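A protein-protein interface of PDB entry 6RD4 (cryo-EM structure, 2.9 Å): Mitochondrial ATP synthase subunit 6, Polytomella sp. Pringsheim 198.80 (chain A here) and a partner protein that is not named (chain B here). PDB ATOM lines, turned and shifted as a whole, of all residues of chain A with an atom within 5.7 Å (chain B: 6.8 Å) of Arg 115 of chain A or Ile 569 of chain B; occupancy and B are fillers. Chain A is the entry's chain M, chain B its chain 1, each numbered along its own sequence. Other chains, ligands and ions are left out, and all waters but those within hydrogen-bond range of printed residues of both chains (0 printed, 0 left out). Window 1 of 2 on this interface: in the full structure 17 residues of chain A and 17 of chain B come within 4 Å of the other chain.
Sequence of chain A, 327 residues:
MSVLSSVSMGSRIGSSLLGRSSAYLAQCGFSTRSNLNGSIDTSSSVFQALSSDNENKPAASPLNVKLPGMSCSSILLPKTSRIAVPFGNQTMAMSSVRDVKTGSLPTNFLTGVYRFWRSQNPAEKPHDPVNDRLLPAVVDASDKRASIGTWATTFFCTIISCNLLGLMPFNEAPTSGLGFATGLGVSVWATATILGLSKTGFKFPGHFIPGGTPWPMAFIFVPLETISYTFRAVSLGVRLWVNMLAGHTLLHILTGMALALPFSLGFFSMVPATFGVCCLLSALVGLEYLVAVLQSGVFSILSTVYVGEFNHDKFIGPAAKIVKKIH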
ATOM      1  N   LEU A 110      33.146  21.108  20.528  1.00  0.00           N
ATOM      2  CA  LEU A 110      32.456  22.056  19.670  1.00  0.00           C
ATOM      3  C   LEU A 110      30.954  22.074  19.858  1.00  0.00           C
ATOM      4  O   LEU A 110      30.323  23.041  19.453  1.00  0.00           O
ATOM      5  CB  LEU A 110      32.752  21.776  18.209  1.00  0.00           C
ATOM      6  CG  LEU A 110      33.705  22.729  17.508  1.00  0.00           C
ATOM      7  CD1 LEU A 110      33.122  24.108  17.590  1.00  0.00           C
ATOM      8  CD2 LEU A 110      35.073  22.710  18.103  1.00  0.00           C
ATOM      9  N   THR A 111      30.352  21.028  20.407  1.00  0.00           N
ATOM     10  CA  THR A 111      28.946  21.108  20.779  1.00  0.00           C
ATOM     11  C   THR A 111      28.766  22.032  21.956  1.00  0.00           C
ATOM     12  O   THR A 111      27.876  22.874  21.964  1.00  0.00           O
ATOM     13  CB  THR A 111      28.410  19.742  21.143  1.00  0.00           C
ATOM     14  OG1 THR A 111      28.698  18.834  20.092  1.00  0.00           O
ATOM     15  CG2 THR A 111      26.950  19.803  21.341  1.00  0.00           C
ATOM     16  N   GLY A 112      29.617  21.897  22.959  1.00  0.00           N
ATOM     17  CA  GLY A 112      29.510  22.753  24.112  1.00  0.00           C
ATOM     18  C   GLY A 112      29.928  24.171  23.835  1.00  0.00           C
ATOM     19  O   GLY A 112      29.438  25.090  24.478  1.00  0.00           O
ATOM     20  N   VAL A 113      30.833  24.371  22.887  1.00  0.00           N
ATOM     21  CA  VAL A 113      31.253  25.719  22.534  1.00  0.00           C
ATOM     22  C   VAL A 113      30.155  26.424  21.765  1.00  0.00           C
ATOM     23  O   VAL A 113      29.793  27.548  22.098  1.00  0.00           O
ATOM     24  CB  VAL A 113      32.569  25.682  21.752  1.00  0.00           C
ATOM     25  CG1 VAL A 113      32.846  26.994  21.138  1.00  0.00           C
ATOM     26  CG2 VAL A 113      33.678  25.341  22.648  1.00  0.00           C
ATOM     27  N   TYR A 114      29.571  25.760  20.767  1.00  0.00           N
ATOM     28  CA  TYR A 114      28.485  26.346  19.990  1.00  0.00           C
ATOM     29  C   TYR A 114      27.268  26.636  20.843  1.00  0.00           C
ATOM     30  O   TYR A 114      26.656  27.690  20.709  1.00  0.00           O
ATOM     31  CB  TYR A 114      28.069  25.418  18.853  1.00  0.00           C
ATOM     32  CG  TYR A 114      26.879  25.948  18.098  1.00  0.00           C
ATOM     33  CD1 TYR A 114      27.030  26.985  17.211  1.00  0.00           C
ATOM     34  CD2 TYR A 114      25.609  25.416  18.279  1.00  0.00           C
ATOM     35  CE1 TYR A 114      25.981  27.482  16.546  1.00  0.00           C
ATOM     36  CE2 TYR A 114      24.549  25.923  17.615  1.00  0.00           C
ATOM     37  CZ  TYR A 114      24.744  26.959  16.755  1.00  0.00           C
ATOM     38  OH  TYR A 114      23.688  27.473  16.068  1.00  0.00           O
ATOM     39  N   ARG A 115      26.896  25.708  21.714  1.00  0.00           N
ATOM     40  CA  ARG A 115      25.755  25.906  22.585  1.00  0.00           C
ATOM     41  C   ARG A 115      26.008  26.950  23.646  1.00  0.00           C
ATOM     42  O   ARG A 115      25.055  27.424  24.253  1.00  0.00           O
ATOM     43  CB  ARG A 115      25.389  24.608  23.272  1.00  0.00           C
ATOM     44  CG  ARG A 115      24.727  23.637  22.391  1.00  0.00           C
ATOM     45  CD  ARG A 115      24.590  22.317  23.074  1.00  0.00           C
ATOM     46  NE  ARG A 115      23.820  22.417  24.293  1.00  0.00           N
ATOM     47  CZ  ARG A 115      22.500  22.376  24.337  1.00  0.00           C
ATOM     48  NH1 ARG A 115      21.875  22.472  25.488  1.00  0.00           N
ATOM     49  NH2 ARG A 115      21.803  22.250  23.232  1.00  0.00           N
ATOM     50  N   PHE A 116      27.263  27.286  23.909  1.00  0.00           N
ATOM     51  CA  PHE A 116      27.564  28.396  24.794  1.00  0.00           C
ATOM     52  C   PHE A 116      27.295  29.723  24.116  1.00  0.00           C
ATOM     53  O   PHE A 116      26.606  30.576  24.668  1.00  0.00           O
ATOM     54  CB  PHE A 116      29.010  28.328  25.247  1.00  0.00           C
ATOM     55  CG  PHE A 116      29.381  29.393  26.214  1.00  0.00           C
ATOM     56  CD1 PHE A 116      28.998  29.306  27.525  1.00  0.00           C
ATOM     57  CD2 PHE A 116      30.119  30.475  25.821  1.00  0.00           C
ATOM     58  CE1 PHE A 116      29.334  30.282  28.406  1.00  0.00           C
ATOM     59  CE2 PHE A 116      30.452  31.443  26.702  1.00  0.00           C
ATOM     60  CZ  PHE A 116      30.063  31.347  27.987  1.00  0.00           C
ATOM     61  N   TRP A 117      27.826  29.919  22.915  1.00  0.00           N
ATOM     62  CA  TRP A 117      27.679  31.200  22.250  1.00  0.00           C
ATOM     63  C   TRP A 117      26.285  31.403  21.724  1.00  0.00           C
ATOM     64  O   TRP A 117      25.857  32.540  21.541  1.00  0.00           O
ATOM     65  CB  TRP A 117      28.676  31.328  21.119  1.00  0.00           C
ATOM     66  CG  TRP A 117      30.043  31.208  21.563  1.00  0.00           C
ATOM     67  CD1 TRP A 117      30.889  30.233  21.257  1.00  0.00           C
ATOM     68  CD2 TRP A 117      30.747  32.107  22.402  1.00  0.00           C
ATOM     69  NE1 TRP A 117      32.082  30.433  21.858  1.00  0.00           N
ATOM     70  CE2 TRP A 117      32.016  31.588  22.577  1.00  0.00           C
ATOM     71  CE3 TRP A 117      30.416  33.290  23.042  1.00  0.00           C
ATOM     72  CZ2 TRP A 117      32.958  32.205  23.344  1.00  0.00           C
ATOM     73  CZ3 TRP A 117      31.336  33.888  23.797  1.00  0.00           C
ATOM     74  CH2 TRP A 117      32.597  33.351  23.950  1.00  0.00           C
ATOM     75  N   ARG A 118      25.569  30.323  21.474  1.00  0.00           N
ATOM     76  CA  ARG A 118      24.162  30.441  21.146  1.00  0.00           C
ATOM     77  C   ARG A 118      23.353  30.864  22.361  1.00  0.00           C
ATOM     78  O   ARG A 118      22.358  31.570  22.224  1.00  0.00           O
ATOM     79  CB  ARG A 118      23.704  29.119  20.554  1.00  0.00           C
ATOM     80  CG  ARG A 118      22.264  28.957  20.247  1.00  0.00           C
ATOM     81  CD  ARG A 118      21.697  30.073  19.432  1.00  0.00           C
ATOM     82  NE  ARG A 118      20.250  29.989  19.316  1.00  0.00           N
ATOM     83  CZ  ARG A 118      19.390  30.328  20.265  1.00  0.00           C
ATOM     84  NH1 ARG A 118      19.798  30.769  21.430  1.00  0.00           N
ATOM     85  NH2 ARG A 118      18.103  30.213  20.049  1.00  0.00           N
ATOM     86  N   SER A 119      23.791  30.515  23.556  1.00  0.00           N
ATOM     87  CA  SER A 119      23.069  30.875  24.762  1.00  0.00           C
ATOM     88  C   SER A 119      23.224  32.331  25.137  1.00  0.00           C
ATOM     89  O   SER A 119      22.564  32.782  26.069  1.00  0.00           O
ATOM     90  CB  SER A 119      23.549  30.035  25.925  1.00  0.00           C
ATOM     91  OG  SER A 119      24.830  30.450  26.321  1.00  0.00           O
ATOM     92  N   GLU B 565      19.355  24.961  12.927  1.00  0.00           N
ATOM     93  CA  GLU B 565      20.163  23.978  13.627  1.00  0.00           C
ATOM     94  C   GLU B 565      20.137  24.168  15.128  1.00  0.00           C
ATOM     95  O   GLU B 565      20.608  23.302  15.858  1.00  0.00           O
ATOM     96  CB  GLU B 565      21.604  24.014  13.142  1.00  0.00           C
ATOM     97  CG  GLU B 565      22.340  25.251  13.520  1.00  0.00           C
ATOM     98  CD  GLU B 565      22.296  26.292  12.451  1.00  0.00           C
ATOM     99  OE1 GLU B 565      21.583  26.084  11.459  1.00  0.00           O
ATOM    100  OE2 GLU B 565      22.956  27.333  12.598  1.00  0.00           O
ATOM    101  N   ASP B 566      19.605  25.271  15.613  1.00  0.00           N
ATOM    102  CA  ASP B 566      19.414  25.478  17.030  1.00  0.00           C
ATOM    103  C   ASP B 566      17.945  25.489  17.407  1.00  0.00           C
ATOM    104  O   ASP B 566      17.565  26.186  18.338  1.00  0.00           O
ATOM    105  CB  ASP B 566      20.064  26.782  17.453  1.00  0.00           C
ATOM    106  CG  ASP B 566      19.538  27.959  16.689  1.00  0.00           C
ATOM    107  OD1 ASP B 566      19.251  27.819  15.491  1.00  0.00           O
ATOM    108  OD2 ASP B 566      19.414  29.039  17.283  1.00  0.00           O
ATOM    109  N   PHE B 567      17.109  24.726  16.704  1.00  0.00           N
ATOM    110  CA  PHE B 567      15.675  24.831  16.928  1.00  0.00           C
ATOM    111  C   PHE B 567      15.266  24.252  18.264  1.00  0.00           C
ATOM    112  O   PHE B 567      14.335  24.754  18.883  1.00  0.00           O
ATOM    113  CB  PHE B 567      14.895  24.143  15.823  1.00  0.00           C
ATOM    114  CG  PHE B 567      13.431  24.417  15.874  1.00  0.00           C
ATOM    115  CD1 PHE B 567      12.960  25.708  15.815  1.00  0.00           C
ATOM    116  CD2 PHE B 567      12.524  23.390  15.970  1.00  0.00           C
ATOM    117  CE1 PHE B 567      11.616  25.968  15.864  1.00  0.00           C
ATOM    118  CE2 PHE B 567      11.188  23.644  16.020  1.00  0.00           C
ATOM    119  CZ  PHE B 567      10.732  24.932  15.961  1.00  0.00           C
ATOM    120  N   ASP B 568      15.948  23.229  18.739  1.00  0.00           N
ATOM    121  CA  ASP B 568      15.659  22.768  20.079  1.00  0.00           C
ATOM    122  C   ASP B 568      16.238  23.675  21.150  1.00  0.00           C
ATOM    123  O   ASP B 568      15.825  23.580  22.304  1.00  0.00           O
ATOM    124  CB  ASP B 568      16.165  21.350  20.269  1.00  0.00           C
ATOM    125  CG  ASP B 568      17.650  21.268  20.365  1.00  0.00           C
ATOM    126  OD1 ASP B 568      18.342  21.627  19.403  1.00  0.00           O
ATOM    127  OD2 ASP B 568      18.132  20.827  21.420  1.00  0.00           O
ATOM    128  N   ILE B 569      17.200  24.527  20.813  1.00  0.00           N
ATOM    129  CA  ILE B 569      17.637  25.537  21.761  1.00  0.00           C
ATOM    130  C   ILE B 569      16.687  26.702  21.730  1.00  0.00           C
ATOM    131  O   ILE B 569      16.500  27.377  22.735  1.00  0.00           O
ATOM    132  CB  ILE B 569      19.076  25.991  21.472  1.00  0.00           C
ATOM    133  CG1 ILE B 569      19.933  24.816  21.057  1.00  0.00           C
ATOM    134  CG2 ILE B 569      19.698  26.598  22.687  1.00  0.00           C
ATOM    135  CD1 ILE B 569      21.311  25.204  20.685  1.00  0.00           C
ATOM    136  N   THR B 570      16.079  26.964  20.577  1.00  0.00           N
ATOM    137  CA  THR B 570      15.087  28.021  20.474  1.00  0.00           C
ATOM    138  C   THR B 570      13.844  27.676  21.266  1.00  0.00           C
ATOM    139  O   THR B 570      13.368  28.493  22.046  1.00  0.00           O
ATOM    140  CB  THR B 570      14.758  28.261  19.011  1.00  0.00           C
ATOM    141  OG1 THR B 570      15.865  28.898  18.382  1.00  0.00           O
ATOM    142  CG2 THR B 570      13.567  29.116  18.861  1.00  0.00           C
ATOM    143  N   LEU B 571      13.348  26.452  21.138  1.00  0.00           N
ATOM    144  CA  LEU B 571      12.216  26.000  21.931  1.00  0.00           C
ATOM    145  C   LEU B 571      12.536  25.873  23.405  1.00  0.00           C
ATOM    146  O   LEU B 571      11.618  25.873  24.216  1.00  0.00           O
ATOM    147  CB  LEU B 571      11.716  24.657  21.429  1.00  0.00           C
ATOM    148  CG  LEU B 571      11.158  24.647  20.029  1.00  0.00           C
ATOM    149  CD1 LEU B 571      10.935  23.256  19.613  1.00  0.00           C
ATOM    150  CD2 LEU B 571       9.888  25.407  19.976  1.00  0.00           C
ATOM    151  N   ASP B 572      13.795  25.739  23.782  1.00  0.00           N
ATOM    152  CA  ASP B 572      14.154  25.780  25.189  1.00  0.00           C
ATOM    153  C   ASP B 572      14.314  27.187  25.712  1.00  0.00           C
ATOM    154  O   ASP B 572      14.171  27.402  26.917  1.00  0.00           O
ATOM    155  CB  ASP B 572      15.460  25.040  25.439  1.00  0.00           C
ATOM    156  CG  ASP B 572      15.294  23.557  25.407  1.00  0.00           C
ATOM    157  OD1 ASP B 572      14.196  23.104  25.056  1.00  0.00           O
ATOM    158  OD2 ASP B 572      16.255  22.835  25.732  1.00  0.00           O
ATOM    159  N   ASP B 573      14.649  28.137  24.847  1.00  0.00           N
ATOM    160  CA  ASP B 573      14.708  29.528  25.265  1.00  0.00           C
ATOM    161  C   ASP B 573      13.320  30.062  25.546  1.00  0.00           C
ATOM    162  O   ASP B 573      13.107  30.758  26.539  1.00  0.00           O
ATOM    163  CB  ASP B 573      15.388  30.371  24.196  1.00  0.00           C
ATOM    164  CG  ASP B 573      16.860  30.122  24.114  1.00  0.00           C
ATOM    165  OD1 ASP B 573      17.417  29.536  25.054  1.00  0.00           O
ATOM    166  OD2 ASP B 573      17.473  30.509  23.109  1.00  0.00           O
ATOM    167  N   MET B 574      12.358  29.738  24.697  1.00  0.00           N
ATOM    168  CA  MET B 574      11.008  30.219  24.879  1.00  0.00           C
ATOM    169  C   MET B 574      10.155  29.266  25.682  1.00  0.00           C
ATOM    170  O   MET B 574       8.928  29.362  25.629  1.00  0.00           O
ATOM    171  CB  MET B 574      10.364  30.519  23.532  1.00  0.00           C
ATOM    172  CG  MET B 574      10.334  29.422  22.578  1.00  0.00           C
ATOM    173  SD  MET B 574       9.872  30.006  20.962  1.00  0.00           S
ATOM    174  CE  MET B 574      10.845  31.477  20.836  1.00  0.00           C
ATOM    175  N   LYS B 580       8.607  21.144  22.243  1.00  0.00           N
ATOM    176  CA  LYS B 580       9.811  20.333  22.235  1.00  0.00           C
ATOM    177  C   LYS B 580       9.478  18.855  22.187  1.00  0.00           C
ATOM    178  O   LYS B 580      10.185  18.093  21.536  1.00  0.00           O
ATOM    179  CB  LYS B 580      10.645  20.655  23.467  1.00  0.00           C
ATOM    180  CG  LYS B 580      11.932  19.920  23.606  1.00  0.00           C
ATOM    181  CD  LYS B 580      12.991  20.500  22.737  1.00  0.00           C
ATOM    182  CE  LYS B 580      14.346  20.022  23.182  1.00  0.00           C
ATOM    183  NZ  LYS B 580      14.659  20.482  24.548  1.00  0.00           N
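The side-chain carboxylate (OD2) of Asp 573 of chain B is in salt-bridge range of the guanidinium group (NH1) of Arg 118 of chain A, 2.9 Å away. NH2 of Arg 118 of chain A lies within salt-bridge range of OD2 of Asp 566 of chain B, 3.3 Å away. The side-chain hydroxyl (OG1) of Thr 570 of chain B is in hydrogen-bond range of the guanidinium group (NH2) of Arg 118 of chain A.
The backbone carbonyl oxygen of Asp 566 of chain B lies within hydrogen-bond range of the side-chain hydroxyl of Thr 570 of chain B, 3.2 Å away.
Among the printed residues, pairs that only touch across the chains: Tyr 114 of chain A with Glu 565 of chain B (3.5 Å), Tyr 114 of chain A with Asp 566 of chain B (3.9 Å), Arg 115 of chain A with Ile 569 of chain B (3.8 Å) and Arg 118 of chain A with Ile 569 of chain B (3.9 Å).
Arg 115 of chain A touches just one residue of chain B: Ile 569 (3.8 Å). Ile 569 of chain B touches just these residues of chain A: Arg 115 (3.8 Å) and Arg 118 (3.9 Å). Printed residues of chain B within 4 Å of Tyr 114 of chain A: Glu 565 and Asp 566. Of the printed residues of chain A, Asp 566 of chain B touches Tyr 114 (3.9 Å) and Arg 118 (2.4 Å). Of the printed residues of chain A, Glu 565 of chain B touches Tyr 114. Printed residues of chain A within 4 Å of Thr 570 of chain B: Arg 118 (3.1 Å). Printed residues of chain A within 4 Å of Asp 573 of chain B: Arg 118. Leu 110 of chain A touches none of the printed residues of chain B. The nearest residue of chain B that does not touch Arg 115 of chain A is Asp 568 of chain B (4.3 Å).
Of the 10 printed residues of chain A, 3 touch a printed residue of chain B. Hydrophobic or aromatic side chains of chain A that line the printed part of chain B: Tyr 114. Printed residues of chain B that touch a printed residue of chain A: Glu 565, Asp 566, Ile 569, Thr 570 and Asp 573.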
